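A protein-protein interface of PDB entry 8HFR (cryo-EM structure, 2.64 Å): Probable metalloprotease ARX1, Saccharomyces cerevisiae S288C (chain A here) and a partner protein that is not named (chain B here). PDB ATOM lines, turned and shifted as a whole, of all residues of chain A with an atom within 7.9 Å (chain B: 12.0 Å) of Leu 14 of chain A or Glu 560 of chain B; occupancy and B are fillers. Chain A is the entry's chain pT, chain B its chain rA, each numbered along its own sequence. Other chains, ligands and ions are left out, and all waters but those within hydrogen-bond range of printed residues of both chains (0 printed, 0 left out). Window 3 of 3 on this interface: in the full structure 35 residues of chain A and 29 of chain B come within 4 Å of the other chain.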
ATOM      1  N   GLN A  11     -23.635  -2.574 -14.094  1.00  0.00           N
ATOM      2  CA  GLN A  11     -23.432  -1.361 -14.879  1.00  0.00           C
ATOM      3  C   GLN A  11     -21.960  -1.298 -15.275  1.00  0.00           C
ATOM      4  O   GLN A  11     -21.162  -2.173 -14.926  1.00  0.00           O
ATOM      5  CB  GLN A  11     -23.850  -0.104 -14.109  1.00  0.00           C
ATOM      6  N   ILE A  12     -21.612  -0.248 -16.021  1.00  0.00           N
ATOM      7  CA  ILE A  12     -20.247   0.012 -16.474  1.00  0.00           C
ATOM      8  C   ILE A  12     -20.021   1.520 -16.495  1.00  0.00           C
ATOM      9  O   ILE A  12     -20.908   2.294 -16.118  1.00  0.00           O
ATOM     10  CB  ILE A  12     -19.977  -0.610 -17.855  1.00  0.00           C
ATOM     11  N   LEU A  13     -18.834   1.942 -16.936  1.00  0.00           N
ATOM     12  CA  LEU A  13     -18.467   3.354 -16.994  1.00  0.00           C
ATOM     13  C   LEU A  13     -19.290   4.092 -18.056  1.00  0.00           C
ATOM     14  O   LEU A  13     -20.023   3.497 -18.853  1.00  0.00           O
ATOM     15  CB  LEU A  13     -16.972   3.506 -17.264  1.00  0.00           C
ATOM     16  N   LEU A  14     -19.160   5.423 -18.063  1.00  0.00           N
ATOM     17  CA  LEU A  14     -19.955   6.263 -18.953  1.00  0.00           C
ATOM     18  C   LEU A  14     -19.075   7.247 -19.720  1.00  0.00           C
ATOM     19  O   LEU A  14     -17.845   7.158 -19.666  1.00  0.00           O
ATOM     20  CB  LEU A  14     -21.031   7.007 -18.160  1.00  0.00           C
ATOM     21  N   LYS A  15     -19.694   8.195 -20.426  1.00  0.00           N
ATOM     22  CA  LYS A  15     -19.023   8.995 -21.444  1.00  0.00           C
ATOM     23  C   LYS A  15     -18.956  10.461 -21.022  1.00  0.00           C
ATOM     24  O   LYS A  15     -19.468  10.850 -19.965  1.00  0.00           O
ATOM     25  CB  LYS A  15     -19.738   8.865 -22.797  1.00  0.00           C
ATOM     26  N   ASP A  16     -18.273  11.256 -21.864  1.00  0.00           N
ATOM     27  CA  ASP A  16     -18.284  12.727 -21.847  1.00  0.00           C
ATOM     28  C   ASP A  16     -17.654  13.309 -20.577  1.00  0.00           C
ATOM     29  O   ASP A  16     -18.160  14.271 -19.998  1.00  0.00           O
ATOM     30  CB  ASP A  16     -19.704  13.271 -22.049  1.00  0.00           C
ATOM     31  CG  ASP A  16     -19.723  14.621 -22.739  1.00  0.00           C
ATOM     32  OD1 ASP A  16     -18.712  14.980 -23.382  1.00  0.00           O
ATOM     33  OD2 ASP A  16     -20.757  15.315 -22.639  1.00  0.00           O
ATOM     34  N   LYS A  17     -16.530  12.734 -20.153  1.00  0.00           N
ATOM     35  CA  LYS A  17     -15.842  13.187 -18.951  1.00  0.00           C
ATOM     36  C   LYS A  17     -14.375  13.424 -19.275  1.00  0.00           C
ATOM     37  O   LYS A  17     -13.873  12.987 -20.314  1.00  0.00           O
ATOM     38  CB  LYS A  17     -15.979  12.179 -17.804  1.00  0.00           C
ATOM     39  CG  LYS A  17     -17.408  11.868 -17.395  1.00  0.00           C
ATOM     40  CD  LYS A  17     -17.981  12.971 -16.528  1.00  0.00           C
ATOM     41  CE  LYS A  17     -19.405  13.306 -16.923  1.00  0.00           C
ATOM     42  NZ  LYS A  17     -20.328  12.170 -16.680  1.00  0.00           N
ATOM     43  N   ASN A  18     -13.703  14.137 -18.359  1.00  0.00           N
ATOM     44  CA  ASN A  18     -12.269  14.463 -18.429  1.00  0.00           C
ATOM     45  C   ASN A  18     -11.905  15.249 -19.689  1.00  0.00           C
ATOM     46  O   ASN A  18     -10.845  15.044 -20.281  1.00  0.00           O
ATOM     47  CB  ASN A  18     -11.401  13.210 -18.309  1.00  0.00           C
ATOM     48  CG  ASN A  18     -11.825  12.319 -17.174  1.00  0.00           C
ATOM     49  OD1 ASN A  18     -11.800  12.726 -16.015  1.00  0.00           O
ATOM     50  ND2 ASN A  18     -12.227  11.097 -17.497  1.00  0.00           N
ATOM     51  N   ASN A  85     -23.207  14.440  -6.736  1.00  0.00           N
ATOM     52  CA  ASN A  85     -23.638  13.273  -5.980  1.00  0.00           C
ATOM     53  C   ASN A  85     -22.679  12.893  -4.863  1.00  0.00           C
ATOM     54  O   ASN A  85     -23.122  12.388  -3.826  1.00  0.00           O
ATOM     55  CB  ASN A  85     -23.830  12.082  -6.921  1.00  0.00           C
ATOM     56  N   ARG A 249     -11.011  11.418 -13.282  1.00  0.00           N
ATOM     57  CA  ARG A 249     -12.163  11.443 -12.397  1.00  0.00           C
ATOM     58  C   ARG A 249     -12.359  10.060 -11.796  1.00  0.00           C
ATOM     59  O   ARG A 249     -12.521   9.082 -12.530  1.00  0.00           O
ATOM     60  CB  ARG A 249     -13.402  11.881 -13.165  1.00  0.00           C
ATOM     61  CG  ARG A 249     -14.693  11.721 -12.405  1.00  0.00           C
ATOM     62  CD  ARG A 249     -15.815  12.342 -13.174  1.00  0.00           C
ATOM     63  NE  ARG A 249     -17.074  12.287 -12.454  1.00  0.00           N
ATOM     64  CZ  ARG A 249     -18.076  11.482 -12.775  1.00  0.00           C
ATOM     65  NH1 ARG A 249     -17.959  10.660 -13.801  1.00  0.00           N
ATOM     66  NH2 ARG A 249     -19.192  11.500 -12.068  1.00  0.00           N
ATOM     67  N   PHE A 250     -12.316   9.990 -10.460  1.00  0.00           N
ATOM     68  CA  PHE A 250     -12.312   8.818  -9.572  1.00  0.00           C
ATOM     69  C   PHE A 250     -11.037   7.987  -9.684  1.00  0.00           C
ATOM     70  O   PHE A 250     -10.950   6.964  -9.024  1.00  0.00           O
ATOM     71  CB  PHE A 250     -13.509   7.869  -9.767  1.00  0.00           C
ATOM     72  CG  PHE A 250     -14.840   8.481  -9.454  1.00  0.00           C
ATOM     73  CD1 PHE A 250     -15.122   8.947  -8.189  1.00  0.00           C
ATOM     74  CD2 PHE A 250     -15.814   8.573 -10.429  1.00  0.00           C
ATOM     75  CE1 PHE A 250     -16.348   9.504  -7.903  1.00  0.00           C
ATOM     76  CE2 PHE A 250     -17.040   9.134 -10.148  1.00  0.00           C
ATOM     77  CZ  PHE A 250     -17.302   9.602  -8.883  1.00  0.00           C
ATOM     78  N   LYS B 555     -38.975   6.248 -14.824  1.00  0.00           N
ATOM     79  CA  LYS B 555     -38.562   6.271 -13.425  1.00  0.00           C
ATOM     80  C   LYS B 555     -37.382   5.340 -13.165  1.00  0.00           C
ATOM     81  O   LYS B 555     -36.455   5.694 -12.430  1.00  0.00           O
ATOM     82  CB  LYS B 555     -39.736   5.911 -12.517  1.00  0.00           C
ATOM     83  CG  LYS B 555     -39.451   6.173 -11.051  1.00  0.00           C
ATOM     84  CD  LYS B 555     -40.705   6.101 -10.211  1.00  0.00           C
ATOM     85  CE  LYS B 555     -40.364   6.045  -8.732  1.00  0.00           C
ATOM     86  NZ  LYS B 555     -39.864   7.348  -8.222  1.00  0.00           N
ATOM     87  N   ASN B 556     -37.391   4.145 -13.758  1.00  0.00           N
ATOM     88  CA  ASN B 556     -36.301   3.186 -13.535  1.00  0.00           C
ATOM     89  C   ASN B 556     -35.143   3.458 -14.498  1.00  0.00           C
ATOM     90  O   ASN B 556     -34.866   2.681 -15.414  1.00  0.00           O
ATOM     91  CB  ASN B 556     -36.797   1.757 -13.713  1.00  0.00           C
ATOM     92  CG  ASN B 556     -37.716   1.309 -12.606  1.00  0.00           C
ATOM     93  OD1 ASN B 556     -37.544   1.688 -11.450  1.00  0.00           O
ATOM     94  ND2 ASN B 556     -38.691   0.479 -12.950  1.00  0.00           N
ATOM     95  N   ARG B 557     -34.447   4.582 -14.288  1.00  0.00           N
ATOM     96  CA  ARG B 557     -33.520   4.952 -15.355  1.00  0.00           C
ATOM     97  C   ARG B 557     -32.126   4.328 -15.297  1.00  0.00           C
ATOM     98  O   ARG B 557     -31.902   3.287 -15.923  1.00  0.00           O
ATOM     99  CB  ARG B 557     -33.363   6.471 -15.385  1.00  0.00           C
ATOM    100  N   TYR B 558     -31.181   4.913 -14.548  1.00  0.00           N
ATOM    101  CA  TYR B 558     -29.835   4.341 -14.604  1.00  0.00           C
ATOM    102  C   TYR B 558     -28.952   4.406 -13.358  1.00  0.00           C
ATOM    103  O   TYR B 558     -28.326   3.405 -12.999  1.00  0.00           O
ATOM    104  CB  TYR B 558     -29.058   4.972 -15.760  1.00  0.00           C
ATOM    105  CG  TYR B 558     -27.711   4.328 -15.970  1.00  0.00           C
ATOM    106  CD1 TYR B 558     -27.590   2.947 -16.079  1.00  0.00           C
ATOM    107  CD2 TYR B 558     -26.562   5.095 -16.059  1.00  0.00           C
ATOM    108  CE1 TYR B 558     -26.366   2.352 -16.255  1.00  0.00           C
ATOM    109  CE2 TYR B 558     -25.330   4.510 -16.246  1.00  0.00           C
ATOM    110  CZ  TYR B 558     -25.236   3.138 -16.342  1.00  0.00           C
ATOM    111  OH  TYR B 558     -24.005   2.548 -16.528  1.00  0.00           O
ATOM    112  N   VAL B 559     -28.980   5.544 -12.656  1.00  0.00           N
ATOM    113  CA  VAL B 559     -27.800   6.328 -12.250  1.00  0.00           C
ATOM    114  C   VAL B 559     -26.566   5.538 -11.804  1.00  0.00           C
ATOM    115  O   VAL B 559     -26.651   4.637 -10.961  1.00  0.00           O
ATOM    116  CB  VAL B 559     -28.209   7.314 -11.142  1.00  0.00           C
ATOM    117  CG1 VAL B 559     -27.138   8.375 -10.940  1.00  0.00           C
ATOM    118  CG2 VAL B 559     -29.546   7.948 -11.473  1.00  0.00           C
ATOM    119  N   GLU B 560     -25.403   5.904 -12.360  1.00  0.00           N
ATOM    120  CA  GLU B 560     -24.112   5.253 -12.164  1.00  0.00           C
ATOM    121  C   GLU B 560     -23.334   5.862 -10.992  1.00  0.00           C
ATOM    122  O   GLU B 560     -23.492   7.036 -10.651  1.00  0.00           O
ATOM    123  CB  GLU B 560     -23.270   5.382 -13.430  1.00  0.00           C
ATOM    124  CG  GLU B 560     -22.164   4.366 -13.547  1.00  0.00           C
ATOM    125  CD  GLU B 560     -20.920   4.955 -14.141  1.00  0.00           C
ATOM    126  OE1 GLU B 560     -20.917   6.160 -14.460  1.00  0.00           O
ATOM    127  OE2 GLU B 560     -19.926   4.219 -14.232  1.00  0.00           O
ATOM    128  N   ARG B 561     -22.454   5.051 -10.395  1.00  0.00           N
ATOM    129  CA  ARG B 561     -21.634   5.444  -9.260  1.00  0.00           C
ATOM    130  C   ARG B 561     -20.142   5.308  -9.555  1.00  0.00           C
ATOM    131  O   ARG B 561     -19.710   4.624 -10.495  1.00  0.00           O
ATOM    132  CB  ARG B 561     -21.974   4.608  -8.020  1.00  0.00           C
ATOM    133  CG  ARG B 561     -23.100   5.162  -7.165  1.00  0.00           C
ATOM    134  CD  ARG B 561     -24.442   4.584  -7.564  1.00  0.00           C
ATOM    135  NE  ARG B 561     -24.394   3.132  -7.704  1.00  0.00           N
ATOM    136  CZ  ARG B 561     -24.710   2.266  -6.745  1.00  0.00           C
ATOM    137  NH1 ARG B 561     -25.108   2.699  -5.557  1.00  0.00           N
ATOM    138  NH2 ARG B 561     -24.631   0.964  -6.976  1.00  0.00           N
ATOM    139  N   GLY B 562     -19.349   5.959  -8.696  1.00  0.00           N
ATOM    140  CA  GLY B 562     -17.904   5.877  -8.804  1.00  0.00           C
ATOM    141  C   GLY B 562     -17.356   4.494  -8.523  1.00  0.00           C
ATOM    142  O   GLY B 562     -16.292   4.132  -9.024  1.00  0.00           O
ATOM    143  N   SER B 563     -18.076   3.702  -7.727  1.00  0.00           N
ATOM    144  CA  SER B 563     -17.706   2.307  -7.537  1.00  0.00           C
ATOM    145  C   SER B 563     -17.882   1.517  -8.822  1.00  0.00           C
ATOM    146  O   SER B 563     -17.115   0.592  -9.098  1.00  0.00           O
ATOM    147  CB  SER B 563     -18.538   1.692  -6.417  1.00  0.00           C
ATOM    148  OG  SER B 563     -19.915   1.734  -6.736  1.00  0.00           O
ATOM    149  N   ASP B 564     -18.880   1.872  -9.628  1.00  0.00           N
ATOM    150  CA  ASP B 564     -19.035   1.221 -10.920  1.00  0.00           C
ATOM    151  C   ASP B 564     -18.015   1.729 -11.922  1.00  0.00           C
ATOM    152  O   ASP B 564     -17.699   1.028 -12.889  1.00  0.00           O
ATOM    153  CB  ASP B 564     -20.451   1.427 -11.447  1.00  0.00           C
ATOM    154  CG  ASP B 564     -21.427   0.432 -10.875  1.00  0.00           C
ATOM    155  OD1 ASP B 564     -20.976  -0.498 -10.176  1.00  0.00           O
ATOM    156  OD2 ASP B 564     -22.642   0.580 -11.107  1.00  0.00           O
ATOM    157  N   VAL B 565     -17.498   2.944 -11.723  1.00  0.00           N
ATOM    158  CA  VAL B 565     -16.392   3.408 -12.558  1.00  0.00           C
ATOM    159  C   VAL B 565     -15.116   2.635 -12.240  1.00  0.00           C
ATOM    160  O   VAL B 565     -14.502   2.024 -13.121  1.00  0.00           O
ATOM    161  CB  VAL B 565     -16.169   4.921 -12.390  1.00  0.00           C
ATOM    162  CG1 VAL B 565     -15.056   5.379 -13.298  1.00  0.00           C
ATOM    163  CG2 VAL B 565     -17.426   5.678 -12.683  1.00  0.00           C
ATOM    164  N   VAL B 566     -14.701   2.649 -10.973  1.00  0.00           N
ATOM    165  CA  VAL B 566     -13.370   2.177 -10.606  1.00  0.00           C
ATOM    166  C   VAL B 566     -13.323   0.678 -10.301  1.00  0.00           C
ATOM    167  O   VAL B 566     -12.246   0.073 -10.381  1.00  0.00           O
ATOM    168  CB  VAL B 566     -12.843   3.032  -9.431  1.00  0.00           C
ATOM    169  CG1 VAL B 566     -13.484   2.655  -8.136  1.00  0.00           C
ATOM    170  CG2 VAL B 566     -11.337   2.973  -9.309  1.00  0.00           C
ATOM    171  N   PHE B 567     -14.458   0.047 -10.010  1.00  0.00           N
ATOM    172  CA  PHE B 567     -14.475  -1.350  -9.611  1.00  0.00           C
ATOM    173  C   PHE B 567     -15.275  -2.247 -10.538  1.00  0.00           C
ATOM    174  O   PHE B 567     -15.291  -3.462 -10.322  1.00  0.00           O
ATOM    175  CB  PHE B 567     -15.025  -1.492  -8.186  1.00  0.00           C
ATOM    176  CG  PHE B 567     -13.968  -1.466  -7.132  1.00  0.00           C
ATOM    177  CD1 PHE B 567     -13.104  -2.529  -6.978  1.00  0.00           C
ATOM    178  CD2 PHE B 567     -13.834  -0.375  -6.295  1.00  0.00           C
ATOM    179  CE1 PHE B 567     -12.128  -2.502  -6.013  1.00  0.00           C
ATOM    180  CE2 PHE B 567     -12.859  -0.340  -5.333  1.00  0.00           C
ATOM    181  CZ  PHE B 567     -12.007  -1.404  -5.190  1.00  0.00           C
ATOM    182  N   GLY B 568     -15.956  -1.695 -11.537  1.00  0.00           N
ATOM    183  CA  GLY B 568     -16.514  -2.536 -12.580  1.00  0.00           C
ATOM    184  C   GLY B 568     -15.408  -3.137 -13.428  1.00  0.00           C
ATOM    185  O   GLY B 568     -14.390  -2.494 -13.696  1.00  0.00           O
ATOM    186  N   ASP B 569     -15.625  -4.389 -13.850  1.00  0.00           N
ATOM    187  CA  ASP B 569     -14.616  -5.239 -14.494  1.00  0.00           C
ATOM    188  C   ASP B 569     -13.355  -5.360 -13.634  1.00  0.00           C
ATOM    189  O   ASP B 569     -12.237  -5.099 -14.084  1.00  0.00           O
ATOM    190  CB  ASP B 569     -14.281  -4.756 -15.910  1.00  0.00           C
ATOM    191  N   GLN B 570     -13.545  -5.766 -12.380  1.00  0.00           N
ATOM    192  CA  GLN B 570     -12.454  -5.954 -11.436  1.00  0.00           C
ATOM    193  C   GLN B 570     -12.755  -7.169 -10.575  1.00  0.00           C
ATOM    194  O   GLN B 570     -13.903  -7.384 -10.180  1.00  0.00           O
ATOM    195  CB  GLN B 570     -12.257  -4.728 -10.536  1.00  0.00           C
ATOM    196  CG  GLN B 570     -11.625  -3.515 -11.199  1.00  0.00           C
ATOM    197  CD  GLN B 570     -10.121  -3.588 -11.230  1.00  0.00           C
ATOM    198  OE1 GLN B 570      -9.510  -4.281 -10.421  1.00  0.00           O
ATOM    199  NE2 GLN B 570      -9.509  -2.858 -12.152  1.00  0.00           N
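The side-chain hydroxyl (OH) of Tyr 558 of chain B sits at hydrogen-bond distance from the backbone carbonyl oxygen (O) of Ile 12 of chain A, at 3.1 Å.
OE2 of Glu 560 of chain B lies close to O of Ile 12 of chain A (2.9 Å).
Among the printed residues, pairs that only touch across the chains: Gln 11 of chain A with Tyr 558 of chain B (3.6 Å), Gln 11 of chain A with Asp 564 of chain B (3.3 Å), Leu 13 of chain A with Glu 560 of chain B (3.2 Å), Leu 14 of chain A with Glu 560 of chain B (3.8 Å) and Phe 250 of chain A with Gly 562 of chain B (3.6 Å).
Glu 560 of chain B touches just these residues of chain A: Ile 12, Leu 13 and Leu 14.
Gln 11 of chain A touches just these residues of chain B: Tyr 558 (3.6 Å) and Asp 564 (3.3 Å).
Leu 13 of chain A touches just one residue of chain B: Glu 560.
No residue of chain B comes within 4 Å of Lys 17 of chain A.
Of the printed residues of chain B, Phe 250 of chain A touches Gly 562 (3.6 Å).
Of the printed residues of chain A, Asp 564 of chain B touches Gln 11 (3.3 Å).
Printed residues of chain A within 4 Å of Tyr 558 of chain B: Gln 11 (3.6 Å) and Ile 12 (3.1 Å).
Printed residues of chain A within 4 Å of Gly 562 of chain B: Phe 250.
The nearest residue of chain B that does not touch Leu 14 of chain A is Tyr 558 of chain B (5.3 Å).
The nearest residue of chain A that does not touch Glu 560 of chain B is Gln 11 of chain A (4.8 Å).
The nearest printed residue of chain A that does not touch Gly 562 of chain B is Arg 249 of chain A (6.5 Å).
Hydrophobic or aromatic side chains of chain B that line the printed part of chain A: Tyr 558.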
